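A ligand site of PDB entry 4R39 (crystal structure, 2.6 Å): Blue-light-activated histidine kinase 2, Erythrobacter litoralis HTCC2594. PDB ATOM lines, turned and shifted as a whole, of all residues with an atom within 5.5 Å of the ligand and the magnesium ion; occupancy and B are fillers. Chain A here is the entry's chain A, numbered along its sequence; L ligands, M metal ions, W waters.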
ATOM      1  N   SER A  57     -29.118 -27.691  12.828  1.00  0.00           N
ATOM      2  CA  SER A  57     -28.281 -28.440  11.905  1.00  0.00           C
ATOM      3  C   SER A  57     -28.650 -29.931  11.822  1.00  0.00           C
ATOM      4  O   SER A  57     -28.027 -30.663  11.054  1.00  0.00           O
ATOM      5  CB  SER A  57     -26.810 -28.320  12.297  1.00  0.00           C
ATOM      6  OG  SER A  57     -26.315 -27.016  12.045  1.00  0.00           O
ATOM      7  N   ARG A  60     -29.573 -31.313   8.418  1.00  0.00           N
ATOM      8  CA  ARG A  60     -28.422 -31.251   7.556  1.00  0.00           C
ATOM      9  C   ARG A  60     -27.541 -32.476   7.757  1.00  0.00           C
ATOM     10  O   ARG A  60     -26.963 -33.002   6.803  1.00  0.00           O
ATOM     11  CB  ARG A  60     -27.644 -30.021   7.982  1.00  0.00           C
ATOM     12  CG  ARG A  60     -27.032 -29.230   6.889  1.00  0.00           C
ATOM     13  CD  ARG A  60     -25.987 -28.359   7.505  1.00  0.00           C
ATOM     14  NE  ARG A  60     -24.972 -29.226   8.091  1.00  0.00           N
ATOM     15  CZ  ARG A  60     -24.330 -29.005   9.233  1.00  0.00           C
ATOM     16  NH1 ARG A  60     -23.455 -29.906   9.652  1.00  0.00           N
ATOM     17  NH2 ARG A  60     -24.524 -27.907   9.958  1.00  0.00           N
ATOM     18  N   ARG A  61     -27.441 -32.914   9.003  1.00  0.00           N
ATOM     19  CA  ARG A  61     -26.581 -34.030   9.359  1.00  0.00           C
ATOM     20  C   ARG A  61     -27.254 -35.335   8.980  1.00  0.00           C
ATOM     21  O   ARG A  61     -26.600 -36.285   8.548  1.00  0.00           O
ATOM     22  CB  ARG A  61     -26.249 -33.982  10.848  1.00  0.00           C
ATOM     23  CG  ARG A  61     -25.468 -32.735  11.217  1.00  0.00           C
ATOM     24  CD  ARG A  61     -25.174 -32.596  12.689  1.00  0.00           C
ATOM     25  NE  ARG A  61     -24.400 -31.385  12.946  1.00  0.00           N
ATOM     26  CZ  ARG A  61     -24.541 -30.595  14.006  1.00  0.00           C
ATOM     27  NH1 ARG A  61     -25.443 -30.854  14.940  1.00  0.00           N
ATOM     28  NH2 ARG A  61     -23.761 -29.523  14.122  1.00  0.00           N
ATOM     29  N   GLU A 132     -20.302 -29.574   7.916  1.00  0.00           N
ATOM     30  CA  GLU A 132     -20.066 -28.649   9.017  1.00  0.00           C
ATOM     31  C   GLU A 132     -19.458 -27.333   8.557  1.00  0.00           C
ATOM     32  O   GLU A 132     -19.946 -26.258   8.890  1.00  0.00           O
ATOM     33  CB  GLU A 132     -19.129 -29.261  10.051  1.00  0.00           C
ATOM     34  CG  GLU A 132     -19.717 -30.405  10.853  1.00  0.00           C
ATOM     35  CD  GLU A 132     -21.048 -30.050  11.472  1.00  0.00           C
ATOM     36  OE1 GLU A 132     -21.229 -28.886  11.894  1.00  0.00           O
ATOM     37  OE2 GLU A 132     -21.936 -30.937  11.504  1.00  0.00           O
ATOM     38  N   VAL A 133     -18.362 -27.435   7.809  1.00  0.00           N
ATOM     39  CA  VAL A 133     -17.595 -26.266   7.441  1.00  0.00           C
ATOM     40  C   VAL A 133     -18.314 -25.439   6.385  1.00  0.00           C
ATOM     41  O   VAL A 133     -18.287 -24.213   6.421  1.00  0.00           O
ATOM     42  CB  VAL A 133     -16.188 -26.653   6.932  1.00  0.00           C
ATOM     43  CG1 VAL A 133     -15.391 -25.413   6.587  1.00  0.00           C
ATOM     44  CG2 VAL A 133     -15.467 -27.485   7.980  1.00  0.00           C
ATOM     45  N   ASN A 136     -21.255 -23.607   7.736  1.00  0.00           N
ATOM     46  CA  ASN A 136     -20.713 -22.497   8.506  1.00  0.00           C
ATOM     47  C   ASN A 136     -20.456 -21.294   7.613  1.00  0.00           C
ATOM     48  O   ASN A 136     -20.739 -20.166   7.998  1.00  0.00           O
ATOM     49  CB  ASN A 136     -19.427 -22.916   9.213  1.00  0.00           C
ATOM     50  CG  ASN A 136     -19.682 -23.583  10.542  1.00  0.00           C
ATOM     51  OD1 ASN A 136     -20.817 -23.640  11.019  1.00  0.00           O
ATOM     52  ND2 ASN A 136     -18.623 -24.102  11.161  1.00  0.00           N
ATOM     53  N   ALA A 137     -19.925 -21.552   6.421  1.00  0.00           N
ATOM     54  CA  ALA A 137     -19.664 -20.479   5.478  1.00  0.00           C
ATOM     55  C   ALA A 137     -20.956 -19.750   5.141  1.00  0.00           C
ATOM     56  O   ALA A 137     -21.065 -18.538   5.309  1.00  0.00           O
ATOM     57  CB  ALA A 137     -19.021 -21.017   4.222  1.00  0.00           C
ATOM     58  N   GLN A 139     -23.908 -19.862   6.559  1.00  0.00           N
ATOM     59  CA  GLN A 139     -24.680 -19.394   7.707  1.00  0.00           C
ATOM     60  C   GLN A 139     -24.076 -18.154   8.351  1.00  0.00           C
ATOM     61  O   GLN A 139     -24.792 -17.258   8.778  1.00  0.00           O
ATOM     62  CB  GLN A 139     -24.791 -20.481   8.767  1.00  0.00           C
ATOM     63  CG  GLN A 139     -25.862 -21.520   8.490  1.00  0.00           C
ATOM     64  CD  GLN A 139     -25.942 -22.572   9.582  1.00  0.00           C
ATOM     65  OE1 GLN A 139     -25.092 -22.626  10.476  1.00  0.00           O
ATOM     66  NE2 GLN A 139     -26.961 -23.413   9.518  1.00  0.00           N
ATOM     67  N   HIS A 140     -22.748 -18.118   8.425  1.00  0.00           N
ATOM     68  CA  HIS A 140     -22.056 -17.147   9.268  1.00  0.00           C
ATOM     69  C   HIS A 140     -21.222 -16.109   8.505  1.00  0.00           C
ATOM     70  O   HIS A 140     -21.116 -14.958   8.930  1.00  0.00           O
ATOM     71  CB  HIS A 140     -21.148 -17.870  10.268  1.00  0.00           C
ATOM     72  CG  HIS A 140     -21.862 -18.888  11.106  1.00  0.00           C
ATOM     73  ND1 HIS A 140     -22.887 -18.551  11.964  1.00  0.00           N
ATOM     74  CD2 HIS A 140     -21.680 -20.224  11.236  1.00  0.00           C
ATOM     75  CE1 HIS A 140     -23.313 -19.642  12.580  1.00  0.00           C
ATOM     76  NE2 HIS A 140     -22.594 -20.672  12.153  1.00  0.00           N
ATOM     77  N   ALA A 141     -20.616 -16.518   7.389  1.00  0.00           N
ATOM     78  CA  ALA A 141     -19.606 -15.682   6.745  1.00  0.00           C
ATOM     79  C   ALA A 141     -20.179 -14.415   6.110  1.00  0.00           C
ATOM     80  O   ALA A 141     -19.421 -13.495   5.799  1.00  0.00           O
ATOM     81  CB  ALA A 141     -18.846 -16.478   5.690  1.00  0.00           C
ATOM     82  N   ASP A 168     -13.951 -18.787   2.103  1.00  0.00           N
ATOM     83  CA  ASP A 168     -14.859 -17.622   2.078  1.00  0.00           C
ATOM     84  C   ASP A 168     -14.114 -16.378   1.658  1.00  0.00           C
ATOM     85  O   ASP A 168     -12.907 -16.296   1.831  1.00  0.00           O
ATOM     86  CB  ASP A 168     -15.375 -17.279   3.473  1.00  0.00           C
ATOM     87  CG  ASP A 168     -16.183 -18.358   4.086  1.00  0.00           C
ATOM     88  OD1 ASP A 168     -16.964 -18.979   3.353  1.00  0.00           O
ATOM     89  OD2 ASP A 168     -16.033 -18.564   5.307  1.00  0.00           O
ATOM     90  N   ARG A 171     -16.913 -12.603   6.169  1.00  0.00           N
ATOM     91  CA  ARG A 171     -16.784 -11.832   7.390  1.00  0.00           C
ATOM     92  C   ARG A 171     -15.587 -12.242   8.251  1.00  0.00           C
ATOM     93  O   ARG A 171     -15.014 -11.419   8.954  1.00  0.00           O
ATOM     94  CB  ARG A 171     -18.102 -11.983   8.135  1.00  0.00           C
ATOM     95  CG  ARG A 171     -18.162 -11.587   9.580  1.00  0.00           C
ATOM     96  CD  ARG A 171     -19.434 -12.171  10.137  1.00  0.00           C
ATOM     97  NE  ARG A 171     -19.752 -11.703  11.476  1.00  0.00           N
ATOM     98  CZ  ARG A 171     -20.208 -10.489  11.743  1.00  0.00           C
ATOM     99  NH1 ARG A 171     -20.370  -9.607  10.771  1.00  0.00           N
ATOM    100  NH2 ARG A 171     -20.474 -10.143  12.990  1.00  0.00           N
ATOM    101  N   GLY A 172     -15.224 -13.520   8.183  1.00  0.00           N
ATOM    102  CA  GLY A 172     -14.138 -14.051   8.985  1.00  0.00           C
ATOM    103  C   GLY A 172     -14.632 -14.592  10.310  1.00  0.00           C
ATOM    104  O   GLY A 172     -15.619 -14.102  10.854  1.00  0.00           O
ATOM    105  N   ILE A 173     -13.935 -15.601  10.826  1.00  0.00           N
ATOM    106  CA  ILE A 173     -14.245 -16.126  12.161  1.00  0.00           C
ATOM    107  C   ILE A 173     -13.751 -15.131  13.207  1.00  0.00           C
ATOM    108  O   ILE A 173     -12.602 -14.692  13.132  1.00  0.00           O
ATOM    109  CB  ILE A 173     -13.593 -17.512  12.385  1.00  0.00           C
ATOM    110  CG1 ILE A 173     -14.097 -18.499  11.319  1.00  0.00           C
ATOM    111  CG2 ILE A 173     -13.874 -18.005  13.803  1.00  0.00           C
ATOM    112  CD1 ILE A 173     -13.608 -19.928  11.483  1.00  0.00           C
ATOM    113  N   PRO A 174     -14.609 -14.780  14.181  1.00  0.00           N
ATOM    114  CA  PRO A 174     -14.205 -13.845  15.243  1.00  0.00           C
ATOM    115  C   PRO A 174     -12.879 -14.227  15.901  1.00  0.00           C
ATOM    116  O   PRO A 174     -12.589 -15.414  16.035  1.00  0.00           O
ATOM    117  CB  PRO A 174     -15.347 -13.973  16.256  1.00  0.00           C
ATOM    118  CG  PRO A 174     -16.529 -14.317  15.435  1.00  0.00           C
ATOM    119  CD  PRO A 174     -16.014 -15.178  14.315  1.00  0.00           C
ATOM    120  N   CYS A 177     -12.804 -16.249  19.075  1.00  0.00           N
ATOM    121  CA  CYS A 177     -13.181 -17.629  18.801  1.00  0.00           C
ATOM    122  C   CYS A 177     -12.081 -18.369  18.043  1.00  0.00           C
ATOM    123  O   CYS A 177     -11.751 -18.005  16.920  1.00  0.00           O
ATOM    124  CB  CYS A 177     -14.484 -17.689  18.003  1.00  0.00           C
ATOM    125  SG  CYS A 177     -15.182 -19.352  17.878  1.00  0.00           S
ATOM    126  N   TRP A 179     -11.894 -21.360  16.549  1.00  0.00           N
ATOM    127  CA  TRP A 179     -12.548 -22.513  15.948  1.00  0.00           C
ATOM    128  C   TRP A 179     -11.503 -23.376  15.241  1.00  0.00           C
ATOM    129  O   TRP A 179     -10.580 -22.845  14.623  1.00  0.00           O
ATOM    130  CB  TRP A 179     -13.607 -22.014  14.968  1.00  0.00           C
ATOM    131  CG  TRP A 179     -14.452 -23.065  14.343  1.00  0.00           C
ATOM    132  CD1 TRP A 179     -15.681 -23.476  14.755  1.00  0.00           C
ATOM    133  CD2 TRP A 179     -14.134 -23.835  13.192  1.00  0.00           C
ATOM    134  NE1 TRP A 179     -16.151 -24.469  13.929  1.00  0.00           N
ATOM    135  CE2 TRP A 179     -15.217 -24.715  12.956  1.00  0.00           C
ATOM    136  CE3 TRP A 179     -13.038 -23.892  12.331  1.00  0.00           C
ATOM    137  CZ2 TRP A 179     -15.235 -25.612  11.901  1.00  0.00           C
ATOM    138  CZ3 TRP A 179     -13.053 -24.790  11.290  1.00  0.00           C
ATOM    139  CH2 TRP A 179     -14.140 -25.637  11.081  1.00  0.00           C
ATOM    140  N   GLU A 182     -12.676 -23.978  19.917  1.00  0.00           N
ATOM    141  CA  GLU A 182     -13.821 -23.334  20.545  1.00  0.00           C
ATOM    142  C   GLU A 182     -14.956 -23.333  19.545  1.00  0.00           C
ATOM    143  O   GLU A 182     -14.727 -23.297  18.339  1.00  0.00           O
ATOM    144  CB  GLU A 182     -13.487 -21.892  20.939  1.00  0.00           C
ATOM    145  CG  GLU A 182     -12.290 -21.732  21.853  1.00  0.00           C
ATOM    146  CD  GLU A 182     -11.983 -20.269  22.168  1.00  0.00           C
ATOM    147  OE1 GLU A 182     -11.947 -19.461  21.228  1.00  0.00           O
ATOM    148  OE2 GLU A 182     -11.784 -19.948  23.360  1.00  0.00           O
ATOM    149  N   GLY A 183     -16.186 -23.387  20.046  1.00  0.00           N
ATOM    150  CA  GLY A 183     -17.352 -23.286  19.181  1.00  0.00           C
ATOM    151  C   GLY A 183     -18.536 -23.970  19.809  1.00  0.00           C
ATOM    152  O   GLY A 183     -18.568 -24.215  21.011  1.00  0.00           O
ATOM    153  N   ASN A 184     -19.519 -24.290  18.972  1.00  0.00           N
ATOM    154  CA  ASN A 184     -20.714 -24.981  19.434  1.00  0.00           C
ATOM    155  C   ASN A 184     -20.629 -26.428  18.998  1.00  0.00           C
ATOM    156  O   ASN A 184     -19.525 -26.939  18.782  1.00  0.00           O
ATOM    157  CB  ASN A 184     -21.953 -24.251  18.916  1.00  0.00           C
ATOM    158  CG  ASN A 184     -21.925 -22.761  19.257  1.00  0.00           C
ATOM    159  OD1 ASN A 184     -21.449 -22.378  20.331  1.00  0.00           O
ATOM    160  ND2 ASN A 184     -22.408 -21.923  18.357  1.00  0.00           N
ATOM    161  N   LEU A 185     -21.756 -27.117  18.873  1.00  0.00           N
ATOM    162  CA  LEU A 185     -21.705 -28.561  18.679  1.00  0.00           C
ATOM    163  C   LEU A 185     -20.936 -28.908  17.406  1.00  0.00           C
ATOM    164  O   LEU A 185     -20.189 -29.877  17.381  1.00  0.00           O
ATOM    165  CB  LEU A 185     -23.105 -29.177  18.650  1.00  0.00           C
ATOM    166  CG  LEU A 185     -23.171 -30.707  18.782  1.00  0.00           C
ATOM    167  CD1 LEU A 185     -22.289 -31.248  19.903  1.00  0.00           C
ATOM    168  CD2 LEU A 185     -24.612 -31.140  19.001  1.00  0.00           C
ATOM    169  N   GLY A 186     -21.114 -28.094  16.365  1.00  0.00           N
ATOM    170  CA  GLY A 186     -20.419 -28.287  15.111  1.00  0.00           C
ATOM    171  C   GLY A 186     -18.911 -28.419  15.248  1.00  0.00           C
ATOM    172  O   GLY A 186     -18.292 -29.265  14.586  1.00  0.00           O
ATOM    173  N   SER A 187     -18.315 -27.593  16.099  1.00  0.00           N
ATOM    174  CA  SER A 187     -16.864 -27.605  16.291  1.00  0.00           C
ATOM    175  C   SER A 187     -16.373 -28.896  16.921  1.00  0.00           C
ATOM    176  O   SER A 187     -15.267 -29.354  16.637  1.00  0.00           O
ATOM    177  CB  SER A 187     -16.446 -26.422  17.178  1.00  0.00           C
ATOM    178  OG  SER A 187     -16.952 -26.561  18.491  1.00  0.00           O
ATOM    179  N   ARG A 188     -17.196 -29.479  17.788  1.00  0.00           N
ATOM    180  CA  ARG A 188     -16.847 -30.733  18.434  1.00  0.00           C
ATOM    181  C   ARG A 188     -16.904 -31.874  17.414  1.00  0.00           C
ATOM    182  O   ARG A 188     -16.037 -32.743  17.414  1.00  0.00           O
ATOM    183  CB  ARG A 188     -17.801 -31.020  19.590  1.00  0.00           C
ATOM    184  CG  ARG A 188     -17.520 -32.313  20.329  1.00  0.00           C
ATOM    185  CD  ARG A 188     -18.408 -32.459  21.557  1.00  0.00           C
ATOM    186  NE  ARG A 188     -18.223 -31.366  22.505  1.00  0.00           N
ATOM    187  CZ  ARG A 188     -18.874 -31.248  23.660  1.00  0.00           C
ATOM    188  NH1 ARG A 188     -19.780 -32.156  24.001  1.00  0.00           N
ATOM    189  NH2 ARG A 188     -18.637 -30.220  24.457  1.00  0.00           N
ATOM    190  N   THR A 210     -12.572 -16.649   5.697  1.00  0.00           N
ATOM    191  CA  THR A 210     -12.131 -17.845   6.401  1.00  0.00           C
ATOM    192  C   THR A 210     -11.691 -18.915   5.393  1.00  0.00           C
ATOM    193  O   THR A 210     -12.453 -19.273   4.500  1.00  0.00           O
ATOM    194  CB  THR A 210     -13.276 -18.444   7.226  1.00  0.00           C
ATOM    195  OG1 THR A 210     -13.880 -17.419   8.019  1.00  0.00           O
ATOM    196  CG2 THR A 210     -12.787 -19.572   8.115  1.00  0.00           C
HETATM  197  P1  LIG L   1     -23.765 -25.657  14.801  1.00  0.00           P
HETATM  198  O1  LIG L   1     -23.828 -26.707  15.861  1.00  0.00           O
HETATM  199  O2  LIG L   1     -22.445 -25.833  13.948  1.00  0.00           O
HETATM  200  O3  LIG L   1     -25.014 -25.804  13.843  1.00  0.00           O
HETATM  201  P2  LIG L   1     -22.436 -23.192  15.116  1.00  0.00           P
HETATM  202  O4  LIG L   1     -22.654 -21.795  15.565  1.00  0.00           O
HETATM  203  O5  LIG L   1     -22.242 -23.192  13.564  1.00  0.00           O
HETATM  204  N1  LIG L   1     -23.768 -24.126  15.541  1.00  0.00           N
HETATM  205  P3  LIG L   1     -19.777 -23.933  15.074  1.00  0.00           P
HETATM  206  O6  LIG L   1     -19.923 -24.688  13.816  1.00  0.00           O
HETATM  207  O7  LIG L   1     -18.812 -24.579  16.075  1.00  0.00           O
HETATM  208  O8  LIG L   1     -21.168 -23.785  15.832  1.00  0.00           O
HETATM  209  O9  LIG L   1     -19.328 -22.469  14.748  1.00  0.00           O
HETATM  210  C1  LIG L   1     -18.705 -21.678  15.771  1.00  0.00           C
HETATM  211  C2  LIG L   1     -18.897 -20.203  15.469  1.00  0.00           C
HETATM  212  O10 LIG L   1     -17.820 -19.744  14.631  1.00  0.00           O
HETATM  213  C3  LIG L   1     -20.166 -19.822  14.716  1.00  0.00           C
HETATM  214  O11 LIG L   1     -21.256 -19.653  15.617  1.00  0.00           O
HETATM  215  C4  LIG L   1     -19.773 -18.509  14.052  1.00  0.00           C
HETATM  216  O12 LIG L   1     -19.939 -17.411  14.938  1.00  0.00           O
HETATM  217  C5  LIG L   1     -18.279 -18.735  13.751  1.00  0.00           C
HETATM  218  N2  LIG L   1     -17.986 -19.153  12.386  1.00  0.00           N
HETATM  219  C6  LIG L   1     -17.828 -20.440  11.928  1.00  0.00           C
HETATM  220  N3  LIG L   1     -17.559 -20.522  10.648  1.00  0.00           N
HETATM  221  C7  LIG L   1     -17.527 -19.198  10.240  1.00  0.00           C
HETATM  222  C8  LIG L   1     -17.284 -18.606   8.979  1.00  0.00           C
HETATM  223  N4  LIG L   1     -17.023 -19.296   7.872  1.00  0.00           N
HETATM  224  N5  LIG L   1     -17.324 -17.249   8.906  1.00  0.00           N
HETATM  225  C9  LIG L   1     -17.586 -16.555  10.021  1.00  0.00           C
HETATM  226  N6  LIG L   1     -17.831 -17.005  11.253  1.00  0.00           N
HETATM  227  C10 LIG L   1     -17.785 -18.341  11.291  1.00  0.00           C
HETATM  228 MG    MG M   1     -21.514 -24.894  12.465  1.00  0.00          MG
HETATM  229  O   HOH W   1     -21.627 -17.803  17.465  1.00  0.00           O
HETATM  230  O   HOH W   2     -20.724 -26.368  11.250  1.00  0.00           O
HETATM  231  O   HOH W   3     -23.034 -17.118  15.374  1.00  0.00           O
HETATM  232  O   HOH W   4     -15.877 -15.784   7.084  1.00  0.00           O
HETATM  233  O   HOH W   5     -19.164 -14.718  12.808  1.00  0.00           O
HETATM  234  O   HOH W   6     -16.151 -23.303   9.623  1.00  0.00           O
HETATM  235  O   HOH W   7     -16.243 -22.374   7.053  1.00  0.00           O
HETATM  236  O   HOH W   8     -24.634 -25.990  18.468  1.00  0.00           O
HETATM  237  O   HOH W   9     -27.099 -26.657  15.253  1.00  0.00           O
HETATM  238  O   HOH W  10     -23.389 -24.839  11.582  1.00  0.00           O
HETATM  239  O   HOH W  11     -26.097 -23.401  13.281  1.00  0.00           O
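The side-chain hydroxyl (OG) of Ser 57 is in hydrogen-bond range of an oxygen (O3) of the ligand (2.5 Å). O4 of the ligand sits at hydrogen-bond distance from ND2 of Asn 184 (2.8 Å). The indole nitrogen (NE1) of Trp 179 sits at hydrogen-bond distance from an oxygen (O7) of the ligand, at 3.4 Å. The backbone NH of Asn 184 sits at hydrogen-bond distance from an oxygen (O7) of the ligand, 3.0 Å away. The backbone NH of Gly 186 sits at hydrogen-bond distance from an oxygen (O1) of the ligand (3.1 Å). The backbone NH (N) of Ser 187 lies within hydrogen-bond range of an oxygen (O7) of the ligand, at 3.1 Å. The guanidinium group of Arg 61 is in salt-bridge range of an oxygen (O1) of the ligand (3.3 Å). A ring nitrogen (NE2) of His 140 sits close to an oxygen (O5) of the ligand, 2.9 Å away. OD2 of Asp 168 is in hydrogen-bond range of N4 of the ligand, at 2.8 Å.
O of Thr 210 sits at hydrogen-bond distance from N of Asp 168, at 2.9 Å. NH1 of Arg 60 lies within salt-bridge range of OE2 of Glu 132, at 2.6 Å. The side-chain amide nitrogen of Asn 136 lies close to the backbone carbonyl oxygen of Glu 132. The backbone NH (N) of Arg 171 lies within hydrogen-bond range of the backbone carbonyl oxygen (O) of Ala 141 (2.7 Å). The guanidinium group of Arg 60 sits at hydrogen-bond distance from the side-chain hydroxyl of Ser 57, 2.9 Å away. NE of Arg 61 lies within salt-bridge range of OE2 of Glu 132 (2.9 Å). The backbone carbonyl oxygen of Asn 184 is in hydrogen-bond range of the side-chain hydroxyl of Ser 187 (2.6 Å). N of Ile 173 lies within hydrogen-bond range of OG1 of Thr 210 (3.3 Å).
Residues that only touch the ligand: Gly 172 (3.3 Å), Ala 141 (3.5 Å), Thr 210 (3.6 Å), Ile 173 (3.7 Å), Gly 183 (3.7 Å), Leu 185 (3.7 Å), Ala 137 (3.8 Å) and Glu 132 (3.9 Å). Hydrophobic or aromatic side chains within 4 Å of the ligand: His 140, Ala 141, Ile 173, Trp 179 and Leu 185. 17 residues have an atom within 4 Å of the ligand: Ser 57, Arg 61, Glu 132, Asn 136, Ala 137, His 140, Ala 141, Asp 168, Gly 172, Ile 173, Trp 179, Gly 183, Asn 184, Leu 185, Gly 186, Ser 187 and Thr 210.
Of the 25 residues printed, 1 comes within 4 Å of the magnesium ion. The nearest printed residue that does not touch the magnesium ion is Glu 132 (4.04 Å).
The magnesium ion is bound by O2 of the ligand, OD1 of Asn 136, water W2, water W10, O6 of the ligand and O5 of the ligand.
Water W2 lies within hydrogen-bond range of the backbone carbonyl oxygen of Glu 132 (2.5 Å) and the side-chain amide nitrogen of Asn 136 (3.1 Å). Water W10 bridges an oxygen (O3) of the ligand (2.9 Å) and the side-chain amide oxygen of Gln 139 (3.0 Å). Water W11 bridges an oxygen (O3) of the ligand (2.7 Å) and the side-chain amide oxygen (OE1) of Gln 139 (3.1 Å). Water W4 lies within hydrogen-bond range of the backbone NH (N) of Gly 172, the side-chain hydroxyl (OG1) of Thr 210, a nitrogen (N5) of the ligand, the side-chain carboxylate (OD2) of Asp 168 and the backbone NH (N) of Arg 171. Water W8 lies within hydrogen-bond range of an oxygen (O1) of the ligand and the backbone NH of Leu 185. Water W5 lies within hydrogen-bond range of a nitrogen (N6) of the ligand (3.1 Å) and the guanidinium group (NE) of Arg 171 (3.3 Å).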
